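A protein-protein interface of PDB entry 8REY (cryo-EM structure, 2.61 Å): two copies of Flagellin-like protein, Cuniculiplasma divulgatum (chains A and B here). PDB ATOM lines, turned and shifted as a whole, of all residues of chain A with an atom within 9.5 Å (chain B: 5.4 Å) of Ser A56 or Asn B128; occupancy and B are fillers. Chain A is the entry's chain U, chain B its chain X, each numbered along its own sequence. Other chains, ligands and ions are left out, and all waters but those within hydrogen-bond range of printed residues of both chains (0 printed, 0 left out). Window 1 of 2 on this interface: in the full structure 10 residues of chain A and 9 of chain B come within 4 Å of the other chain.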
ATOM      1  N   GLU A  37       4.576 -37.768  17.917  1.00  0.00           N
ATOM      2  CA  GLU A  37       3.594 -36.726  18.212  1.00  0.00           C
ATOM      3  C   GLU A  37       2.727 -37.216  19.378  1.00  0.00           C
ATOM      4  O   GLU A  37       2.636 -38.421  19.601  1.00  0.00           O
ATOM      5  CB  GLU A  37       2.805 -36.380  16.940  1.00  0.00           C
ATOM      6  CG  GLU A  37       1.724 -35.316  17.108  1.00  0.00           C
ATOM      7  CD  GLU A  37       2.162 -34.069  17.855  1.00  0.00           C
ATOM      8  OE1 GLU A  37       3.151 -33.429  17.431  1.00  0.00           O
ATOM      9  OE2 GLU A  37       1.547 -33.765  18.897  1.00  0.00           O
ATOM     10  N   THR A  38       2.136 -36.305  20.168  1.00  0.00           N
ATOM     11  CA  THR A  38       1.390 -36.698  21.359  1.00  0.00           C
ATOM     12  C   THR A  38       0.384 -35.599  21.673  1.00  0.00           C
ATOM     13  O   THR A  38       0.763 -34.441  21.771  1.00  0.00           O
ATOM     14  CB  THR A  38       2.322 -36.880  22.567  1.00  0.00           C
ATOM     15  OG1 THR A  38       3.363 -37.797  22.236  1.00  0.00           O
ATOM     16  CG2 THR A  38       1.636 -37.371  23.826  1.00  0.00           C
ATOM     17  N   ALA A  39      -0.893 -35.961  21.832  1.00  0.00           N
ATOM     18  CA  ALA A  39      -1.932 -34.957  22.027  1.00  0.00           C
ATOM     19  C   ALA A  39      -2.916 -35.372  23.120  1.00  0.00           C
ATOM     20  O   ALA A  39      -3.235 -36.550  23.270  1.00  0.00           O
ATOM     21  CB  ALA A  39      -2.632 -34.697  20.715  1.00  0.00           C
ATOM     22  N   GLY A  40      -3.395 -34.381  23.882  1.00  0.00           N
ATOM     23  CA  GLY A  40      -4.553 -34.546  24.743  1.00  0.00           C
ATOM     24  C   GLY A  40      -5.818 -34.359  23.914  1.00  0.00           C
ATOM     25  O   GLY A  40      -6.079 -33.253  23.438  1.00  0.00           O
ATOM     26  N   VAL A  41      -6.559 -35.457  23.712  1.00  0.00           N
ATOM     27  CA  VAL A  41      -7.748 -35.474  22.873  1.00  0.00           C
ATOM     28  C   VAL A  41      -8.892 -36.099  23.666  1.00  0.00           C
ATOM     29  O   VAL A  41      -8.693 -37.094  24.356  1.00  0.00           O
ATOM     30  CB  VAL A  41      -7.517 -36.212  21.536  1.00  0.00           C
ATOM     31  CG1 VAL A  41      -8.756 -36.189  20.657  1.00  0.00           C
ATOM     32  CG2 VAL A  41      -6.345 -35.634  20.758  1.00  0.00           C
ATOM     33  N   THR A  42     -10.090 -35.507  23.563  1.00  0.00           N
ATOM     34  CA  THR A  42     -11.308 -36.079  24.127  1.00  0.00           C
ATOM     35  C   THR A  42     -12.380 -36.140  23.044  1.00  0.00           C
ATOM     36  O   THR A  42     -12.372 -35.335  22.115  1.00  0.00           O
ATOM     37  CB  THR A  42     -11.809 -35.304  25.355  1.00  0.00           C
ATOM     38  OG1 THR A  42     -12.140 -33.965  24.981  1.00  0.00           O
ATOM     39  CG2 THR A  42     -10.825 -35.302  26.503  1.00  0.00           C
ATOM     40  N   ASN A  53     -12.319 -32.855  20.578  1.00  0.00           N
ATOM     41  CA  ASN A  53     -11.857 -31.613  21.167  1.00  0.00           C
ATOM     42  C   ASN A  53     -10.431 -31.817  21.647  1.00  0.00           C
ATOM     43  O   ASN A  53     -10.189 -32.742  22.406  1.00  0.00           O
ATOM     44  CB  ASN A  53     -12.715 -31.222  22.364  1.00  0.00           C
ATOM     45  CG  ASN A  53     -14.123 -30.836  21.984  1.00  0.00           C
ATOM     46  OD1 ASN A  53     -14.400 -30.441  20.849  1.00  0.00           O
ATOM     47  ND2 ASN A  53     -15.013 -30.937  22.947  1.00  0.00           N
ATOM     48  N   VAL A  54      -9.519 -30.920  21.246  1.00  0.00           N
ATOM     49  CA  VAL A  54      -8.098 -31.049  21.544  1.00  0.00           C
ATOM     50  C   VAL A  54      -7.705 -30.072  22.654  1.00  0.00           C
ATOM     51  O   VAL A  54      -7.993 -28.885  22.561  1.00  0.00           O
ATOM     52  CB  VAL A  54      -7.243 -30.817  20.283  1.00  0.00           C
ATOM     53  CG1 VAL A  54      -5.766 -31.029  20.562  1.00  0.00           C
ATOM     54  CG2 VAL A  54      -7.679 -31.708  19.133  1.00  0.00           C
ATOM     55  N   SER A  55      -6.972 -30.554  23.672  1.00  0.00           N
ATOM     56  CA  SER A  55      -6.605 -29.747  24.833  1.00  0.00           C
ATOM     57  C   SER A  55      -5.143 -29.289  24.807  1.00  0.00           C
ATOM     58  O   SER A  55      -4.823 -28.236  25.363  1.00  0.00           O
ATOM     59  CB  SER A  55      -6.920 -30.480  26.111  1.00  0.00           C
ATOM     60  OG  SER A  55      -6.104 -31.633  26.231  1.00  0.00           O
ATOM     61  N   SER A  56      -4.261 -30.096  24.193  1.00  0.00           N
ATOM     62  CA  SER A  56      -2.843 -29.800  24.015  1.00  0.00           C
ATOM     63  C   SER A  56      -2.229 -30.732  22.969  1.00  0.00           C
ATOM     64  O   SER A  56      -2.777 -31.794  22.702  1.00  0.00           O
ATOM     65  CB  SER A  56      -2.115 -29.957  25.326  1.00  0.00           C
ATOM     66  OG  SER A  56      -2.292 -31.270  25.840  1.00  0.00           O
ATOM     67  N   SER A  57      -1.072 -30.355  22.402  1.00  0.00           N
ATOM     68  CA  SER A  57      -0.324 -31.222  21.494  1.00  0.00           C
ATOM     69  C   SER A  57       1.176 -30.951  21.610  1.00  0.00           C
ATOM     70  O   SER A  57       1.586 -29.864  22.020  1.00  0.00           O
ATOM     71  CB  SER A  57      -0.795 -31.082  20.063  1.00  0.00           C
ATOM     72  OG  SER A  57      -0.513 -29.783  19.569  1.00  0.00           O
ATOM     73  N   SER A  58       1.992 -31.936  21.215  1.00  0.00           N
ATOM     74  CA  SER A  58       3.444 -31.843  21.278  1.00  0.00           C
ATOM     75  C   SER A  58       3.975 -30.809  20.280  1.00  0.00           C
ATOM     76  O   SER A  58       4.964 -30.131  20.554  1.00  0.00           O
ATOM     77  CB  SER A  58       4.058 -33.198  21.055  1.00  0.00           C
ATOM     78  OG  SER A  58       5.450 -33.178  21.325  1.00  0.00           O
ATOM     79  N   SER A  59       3.306 -30.690  19.124  1.00  0.00           N
ATOM     80  CA  SER A  59       3.617 -29.700  18.099  1.00  0.00           C
ATOM     81  C   SER A  59       2.336 -29.219  17.409  1.00  0.00           C
ATOM     82  O   SER A  59       1.292 -29.862  17.512  1.00  0.00           O
ATOM     83  CB  SER A  59       4.625 -30.252  17.116  1.00  0.00           C
ATOM     84  OG  SER A  59       4.057 -31.266  16.297  1.00  0.00           O
ATOM     85  N   ALA A  60       2.417 -28.074  16.713  1.00  0.00           N
ATOM     86  CA  ALA A  60       1.311 -27.558  15.915  1.00  0.00           C
ATOM     87  C   ALA A  60       1.396 -28.115  14.490  1.00  0.00           C
ATOM     88  O   ALA A  60       2.400 -27.903  13.809  1.00  0.00           O
ATOM     89  CB  ALA A  60       1.349 -26.048  15.928  1.00  0.00           C
ATOM     90  N   ILE A  61       0.338 -28.814  14.035  1.00  0.00           N
ATOM     91  CA  ILE A  61       0.344 -29.523  12.757  1.00  0.00           C
ATOM     92  C   ILE A  61      -0.932 -29.226  11.962  1.00  0.00           C
ATOM     93  O   ILE A  61      -1.973 -28.919  12.537  1.00  0.00           O
ATOM     94  CB  ILE A  61       0.587 -31.036  12.961  1.00  0.00           C
ATOM     95  CG1 ILE A  61      -0.535 -31.716  13.755  1.00  0.00           C
ATOM     96  CG2 ILE A  61       1.953 -31.269  13.593  1.00  0.00           C
ATOM     97  CD1 ILE A  61      -0.313 -33.191  14.036  1.00  0.00           C
ATOM     98  N   PHE A  98      -4.148 -28.272  14.199  1.00  0.00           N
ATOM     99  CA  PHE A  98      -4.378 -29.195  15.295  1.00  0.00           C
ATOM    100  C   PHE A  98      -3.467 -28.830  16.470  1.00  0.00           C
ATOM    101  O   PHE A  98      -2.260 -29.058  16.418  1.00  0.00           O
ATOM    102  CB  PHE A  98      -4.162 -30.601  14.741  1.00  0.00           C
ATOM    103  CG  PHE A  98      -4.509 -31.750  15.647  1.00  0.00           C
ATOM    104  CD1 PHE A  98      -3.580 -32.230  16.562  1.00  0.00           C
ATOM    105  CD2 PHE A  98      -5.735 -32.400  15.541  1.00  0.00           C
ATOM    106  CE1 PHE A  98      -3.877 -33.322  17.369  1.00  0.00           C
ATOM    107  CE2 PHE A  98      -6.026 -33.498  16.340  1.00  0.00           C
ATOM    108  CZ  PHE A  98      -5.100 -33.952  17.259  1.00  0.00           C
ATOM    109  N   THR A  99      -4.072 -28.236  17.514  1.00  0.00           N
ATOM    110  CA  THR A  99      -3.434 -27.716  18.722  1.00  0.00           C
ATOM    111  C   THR A  99      -4.493 -27.620  19.818  1.00  0.00           C
ATOM    112  O   THR A  99      -5.678 -27.749  19.525  1.00  0.00           O
ATOM    113  CB  THR A  99      -2.889 -26.289  18.534  1.00  0.00           C
ATOM    114  OG1 THR A  99      -3.820 -25.467  17.828  1.00  0.00           O
ATOM    115  CG2 THR A  99      -1.555 -26.219  17.828  1.00  0.00           C
ATOM    116  N   GLY A 100      -4.083 -27.373  21.074  1.00  0.00           N
ATOM    117  CA  GLY A 100      -5.040 -27.073  22.134  1.00  0.00           C
ATOM    118  C   GLY A 100      -5.987 -25.938  21.724  1.00  0.00           C
ATOM    119  O   GLY A 100      -5.555 -24.943  21.148  1.00  0.00           O
ATOM    120  N   GLY A 101      -7.288 -26.114  21.984  1.00  0.00           N
ATOM    121  CA  GLY A 101      -8.297 -25.130  21.626  1.00  0.00           C
ATOM    122  C   GLY A 101      -8.982 -25.369  20.277  1.00  0.00           C
ATOM    123  O   GLY A 101      -9.913 -24.634  19.945  1.00  0.00           O
ATOM    124  N   SER A 102      -8.559 -26.387  19.507  1.00  0.00           N
ATOM    125  CA  SER A 102      -9.206 -26.755  18.247  1.00  0.00           C
ATOM    126  C   SER A 102     -10.267 -27.831  18.466  1.00  0.00           C
ATOM    127  O   SER A 102      -9.978 -28.869  19.058  1.00  0.00           O
ATOM    128  CB  SER A 102      -8.201 -27.224  17.226  1.00  0.00           C
ATOM    129  OG  SER A 102      -7.274 -26.197  16.935  1.00  0.00           O
ATOM    130  N   ASP A 103     -11.478 -27.596  17.930  1.00  0.00           N
ATOM    131  CA  ASP A 103     -12.604 -28.521  18.012  1.00  0.00           C
ATOM    132  C   ASP A 103     -13.109 -28.891  16.613  1.00  0.00           C
ATOM    133  O   ASP A 103     -13.169 -28.039  15.729  1.00  0.00           O
ATOM    134  CB  ASP A 103     -13.768 -27.912  18.800  1.00  0.00           C
ATOM    135  CG  ASP A 103     -13.477 -27.491  20.236  1.00  0.00           C
ATOM    136  OD1 ASP A 103     -12.502 -27.995  20.838  1.00  0.00           O
ATOM    137  OD2 ASP A 103     -14.251 -26.662  20.755  1.00  0.00           O
ATOM    138  N   ILE A 130      -1.994 -41.745  16.794  1.00  0.00           N
ATOM    139  CA  ILE A 130      -1.880 -40.728  17.843  1.00  0.00           C
ATOM    140  C   ILE A 130      -3.096 -40.684  18.780  1.00  0.00           C
ATOM    141  O   ILE A 130      -3.001 -40.108  19.865  1.00  0.00           O
ATOM    142  CB  ILE A 130      -1.530 -39.328  17.286  1.00  0.00           C
ATOM    143  CG1 ILE A 130      -2.644 -38.727  16.418  1.00  0.00           C
ATOM    144  CG2 ILE A 130      -0.188 -39.367  16.570  1.00  0.00           C
ATOM    145  CD1 ILE A 130      -2.542 -37.229  16.190  1.00  0.00           C
ATOM    146  N   THR B  35       6.013 -25.593  29.007  1.00  0.00           N
ATOM    147  CA  THR B  35       4.851 -24.805  28.593  1.00  0.00           C
ATOM    148  C   THR B  35       3.672 -24.887  29.573  1.00  0.00           C
ATOM    149  O   THR B  35       2.606 -24.332  29.298  1.00  0.00           O
ATOM    150  CB  THR B  35       4.382 -25.190  27.183  1.00  0.00           C
ATOM    151  OG1 THR B  35       3.995 -26.565  27.188  1.00  0.00           O
ATOM    152  CG2 THR B  35       5.436 -24.952  26.125  1.00  0.00           C
ATOM    153  N   VAL B  36       3.845 -25.575  30.711  1.00  0.00           N
ATOM    154  CA  VAL B  36       2.769 -25.787  31.677  1.00  0.00           C
ATOM    155  C   VAL B  36       2.468 -24.499  32.454  1.00  0.00           C
ATOM    156  O   VAL B  36       3.379 -23.828  32.937  1.00  0.00           O
ATOM    157  CB  VAL B  36       3.076 -26.972  32.617  1.00  0.00           C
ATOM    158  CG1 VAL B  36       1.935 -27.254  33.585  1.00  0.00           C
ATOM    159  CG2 VAL B  36       3.417 -28.236  31.842  1.00  0.00           C
ATOM    160  N   LEU B 123      -9.568 -20.168  27.517  1.00  0.00           N
ATOM    161  CA  LEU B 123      -8.314 -19.426  27.481  1.00  0.00           C
ATOM    162  C   LEU B 123      -7.171 -20.377  27.130  1.00  0.00           C
ATOM    163  O   LEU B 123      -7.043 -21.452  27.722  1.00  0.00           O
ATOM    164  CB  LEU B 123      -8.066 -18.755  28.838  1.00  0.00           C
ATOM    165  CG  LEU B 123      -9.149 -17.791  29.324  1.00  0.00           C
ATOM    166  CD1 LEU B 123      -8.823 -17.287  30.718  1.00  0.00           C
ATOM    167  CD2 LEU B 123      -9.327 -16.621  28.366  1.00  0.00           C
ATOM    168  N   ILE B 124      -6.326 -19.958  26.179  1.00  0.00           N
ATOM    169  CA  ILE B 124      -5.237 -20.777  25.662  1.00  0.00           C
ATOM    170  C   ILE B 124      -3.922 -20.015  25.818  1.00  0.00           C
ATOM    171  O   ILE B 124      -3.842 -18.833  25.488  1.00  0.00           O
ATOM    172  CB  ILE B 124      -5.511 -21.178  24.194  1.00  0.00           C
ATOM    173  CG1 ILE B 124      -6.774 -22.028  24.052  1.00  0.00           C
ATOM    174  CG2 ILE B 124      -4.326 -21.896  23.576  1.00  0.00           C
ATOM    175  CD1 ILE B 124      -7.950 -21.274  23.490  1.00  0.00           C
ATOM    176  N   TYR B 125      -2.888 -20.709  26.300  1.00  0.00           N
ATOM    177  CA  TYR B 125      -1.550 -20.158  26.443  1.00  0.00           C
ATOM    178  C   TYR B 125      -0.523 -21.185  25.966  1.00  0.00           C
ATOM    179  O   TYR B 125      -0.602 -22.350  26.359  1.00  0.00           O
ATOM    180  CB  TYR B 125      -1.324 -19.792  27.909  1.00  0.00           C
ATOM    181  CG  TYR B 125       0.092 -19.412  28.256  1.00  0.00           C
ATOM    182  CD1 TYR B 125       0.602 -18.166  27.923  1.00  0.00           C
ATOM    183  CD2 TYR B 125       0.924 -20.299  28.923  1.00  0.00           C
ATOM    184  CE1 TYR B 125       1.901 -17.804  28.261  1.00  0.00           C
ATOM    185  CE2 TYR B 125       2.222 -19.953  29.271  1.00  0.00           C
ATOM    186  CZ  TYR B 125       2.717 -18.703  28.931  1.00  0.00           C
ATOM    187  OH  TYR B 125       3.992 -18.345  29.271  1.00  0.00           O
ATOM    188  N   LYS B 126       0.395 -20.766  25.077  1.00  0.00           N
ATOM    189  CA  LYS B 126       1.411 -21.616  24.449  1.00  0.00           C
ATOM    190  C   LYS B 126       0.858 -22.953  23.930  1.00  0.00           C
ATOM    191  O   LYS B 126       1.515 -23.993  24.016  1.00  0.00           O
ATOM    192  CB  LYS B 126       2.613 -21.793  25.382  1.00  0.00           C
ATOM    193  CG  LYS B 126       3.400 -20.515  25.593  1.00  0.00           C
ATOM    194  CD  LYS B 126       4.699 -20.737  26.319  1.00  0.00           C
ATOM    195  CE  LYS B 126       5.518 -19.469  26.435  1.00  0.00           C
ATOM    196  NZ  LYS B 126       6.836 -19.716  27.069  1.00  0.00           N
ATOM    197  N   GLY B 127      -0.360 -22.926  23.373  1.00  0.00           N
ATOM    198  CA  GLY B 127      -0.975 -24.095  22.757  1.00  0.00           C
ATOM    199  C   GLY B 127      -1.637 -25.083  23.723  1.00  0.00           C
ATOM    200  O   GLY B 127      -2.111 -26.129  23.282  1.00  0.00           O
ATOM    201  N   ASN B 128      -1.698 -24.758  25.023  1.00  0.00           N
ATOM    202  CA  ASN B 128      -2.404 -25.538  26.033  1.00  0.00           C
ATOM    203  C   ASN B 128      -3.659 -24.786  26.490  1.00  0.00           C
ATOM    204  O   ASN B 128      -3.617 -23.577  26.687  1.00  0.00           O
ATOM    205  CB  ASN B 128      -1.489 -25.796  27.237  1.00  0.00           C
ATOM    206  CG  ASN B 128      -0.218 -26.549  26.904  1.00  0.00           C
ATOM    207  OD1 ASN B 128      -0.235 -27.518  26.151  1.00  0.00           O
ATOM    208  ND2 ASN B 128       0.894 -26.129  27.487  1.00  0.00           N
ATOM    209  N   VAL B 129      -4.779 -25.493  26.694  1.00  0.00           N
ATOM    210  CA  VAL B 129      -5.971 -24.887  27.284  1.00  0.00           C
ATOM    211  C   VAL B 129      -5.763 -24.735  28.794  1.00  0.00           C
ATOM    212  O   VAL B 129      -5.579 -25.734  29.487  1.00  0.00           O
ATOM    213  CB  VAL B 129      -7.232 -25.717  26.959  1.00  0.00           C
ATOM    214  CG1 VAL B 129      -8.470 -25.227  27.699  1.00  0.00           C
ATOM    215  CG2 VAL B 129      -7.498 -25.751  25.467  1.00  0.00           C
ATOM    216  N   ILE B 130      -5.832 -23.496  29.322  1.00  0.00           N
ATOM    217  CA  ILE B 130      -5.618 -23.228  30.746  1.00  0.00           C
ATOM    218  C   ILE B 130      -6.922 -22.998  31.522  1.00  0.00           C
ATOM    219  O   ILE B 130      -6.913 -23.074  32.752  1.00  0.00           O
ATOM    220  CB  ILE B 130      -4.590 -22.099  30.996  1.00  0.00           C
ATOM    221  CG1 ILE B 130      -5.073 -20.725  30.513  1.00  0.00           C
ATOM    222  CG2 ILE B 130      -3.238 -22.481  30.415  1.00  0.00           C
ATOM    223  CD1 ILE B 130      -4.318 -19.539  31.085  1.00  0.00           C
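Among the printed residues, pairs that only touch across the chains: Ser A56 with Asn B128 (3.2 Å), Gly A101 with Val B129 (3.5 Å), Ser A55 with Asn B128 (3.7 Å) and Ser A56 with Gly B127 (3.8 Å).
Of chain B, only Gly B127 (3.8 Å) and Asn B128 (3.2 Å) come within 4 Å of Ser A56. Of chain A, only Ser A55 (3.7 Å) and Ser A56 (3.2 Å) come within 4 Å of Asn B128. Val B129 touches two residues of chain A. Printed residues of chain A within 4 Å of Gly B127: Ser A56 and Gly A100. Of the printed residues of chain B, Gly A100 touches Gly B127 (3.2 Å). Of the printed residues of chain B, Ser A55 touches Asn B128 (3.7 Å) and Val B129 (3.0 Å). Printed residues of chain B within 4 Å of Gly A101: Val B129 (3.5 Å). Ile B124 touches none of the printed residues of chain A. The nearest residue of chain B that does not touch Ser A56 is Val B129 (5.3 Å). The nearest residue of chain A that does not touch Asn B128 is Ser A57 (4.8 Å). The nearest printed residue of chain B that does not touch Ser A55 is Gly B127 (4.02 Å).
The backbone NH of Ser A55 sits at hydrogen-bond distance from the backbone carbonyl oxygen of Gly A40 (2.9 Å). N of Gly A40 lies within hydrogen-bond range of O of Ser A56, at 2.9 Å. The backbone NH (N) of Gly A101 sits at hydrogen-bond distance from the backbone carbonyl oxygen (O) of Val A54 (2.9 Å). The backbone carbonyl oxygen (O) of Thr B35 lies within hydrogen-bond range of the side-chain amide nitrogen (ND2) of Asn B128 (3.1 Å).
The backbone carbonyl oxygen (O) of Ser A55 lies within hydrogen-bond range of the backbone NH (N) of Val B129 (3.0 Å). The backbone carbonyl oxygen (O) of Gly B127 lies within hydrogen-bond range of the backbone NH (N) of Gly A100, 3.2 Å away.
1 position is printed for both chains.
Of the 22 printed residues of chain A, 4 touch a printed residue of chain B. Printed residues of chain A that touch a printed residue of chain B: Ser A55, Ser A56, Gly A100 and Gly A101. Of the 10 printed residues of chain B, 3 touch a printed residue of chain A. Printed residues of chain B that touch a printed residue of chain A: Gly B127, Asn B128 and Val B129. Among the printed residues, no Asp or Glu carboxylate lies within 4 Å of a Lys or Arg side-chain nitrogen of the other chain.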
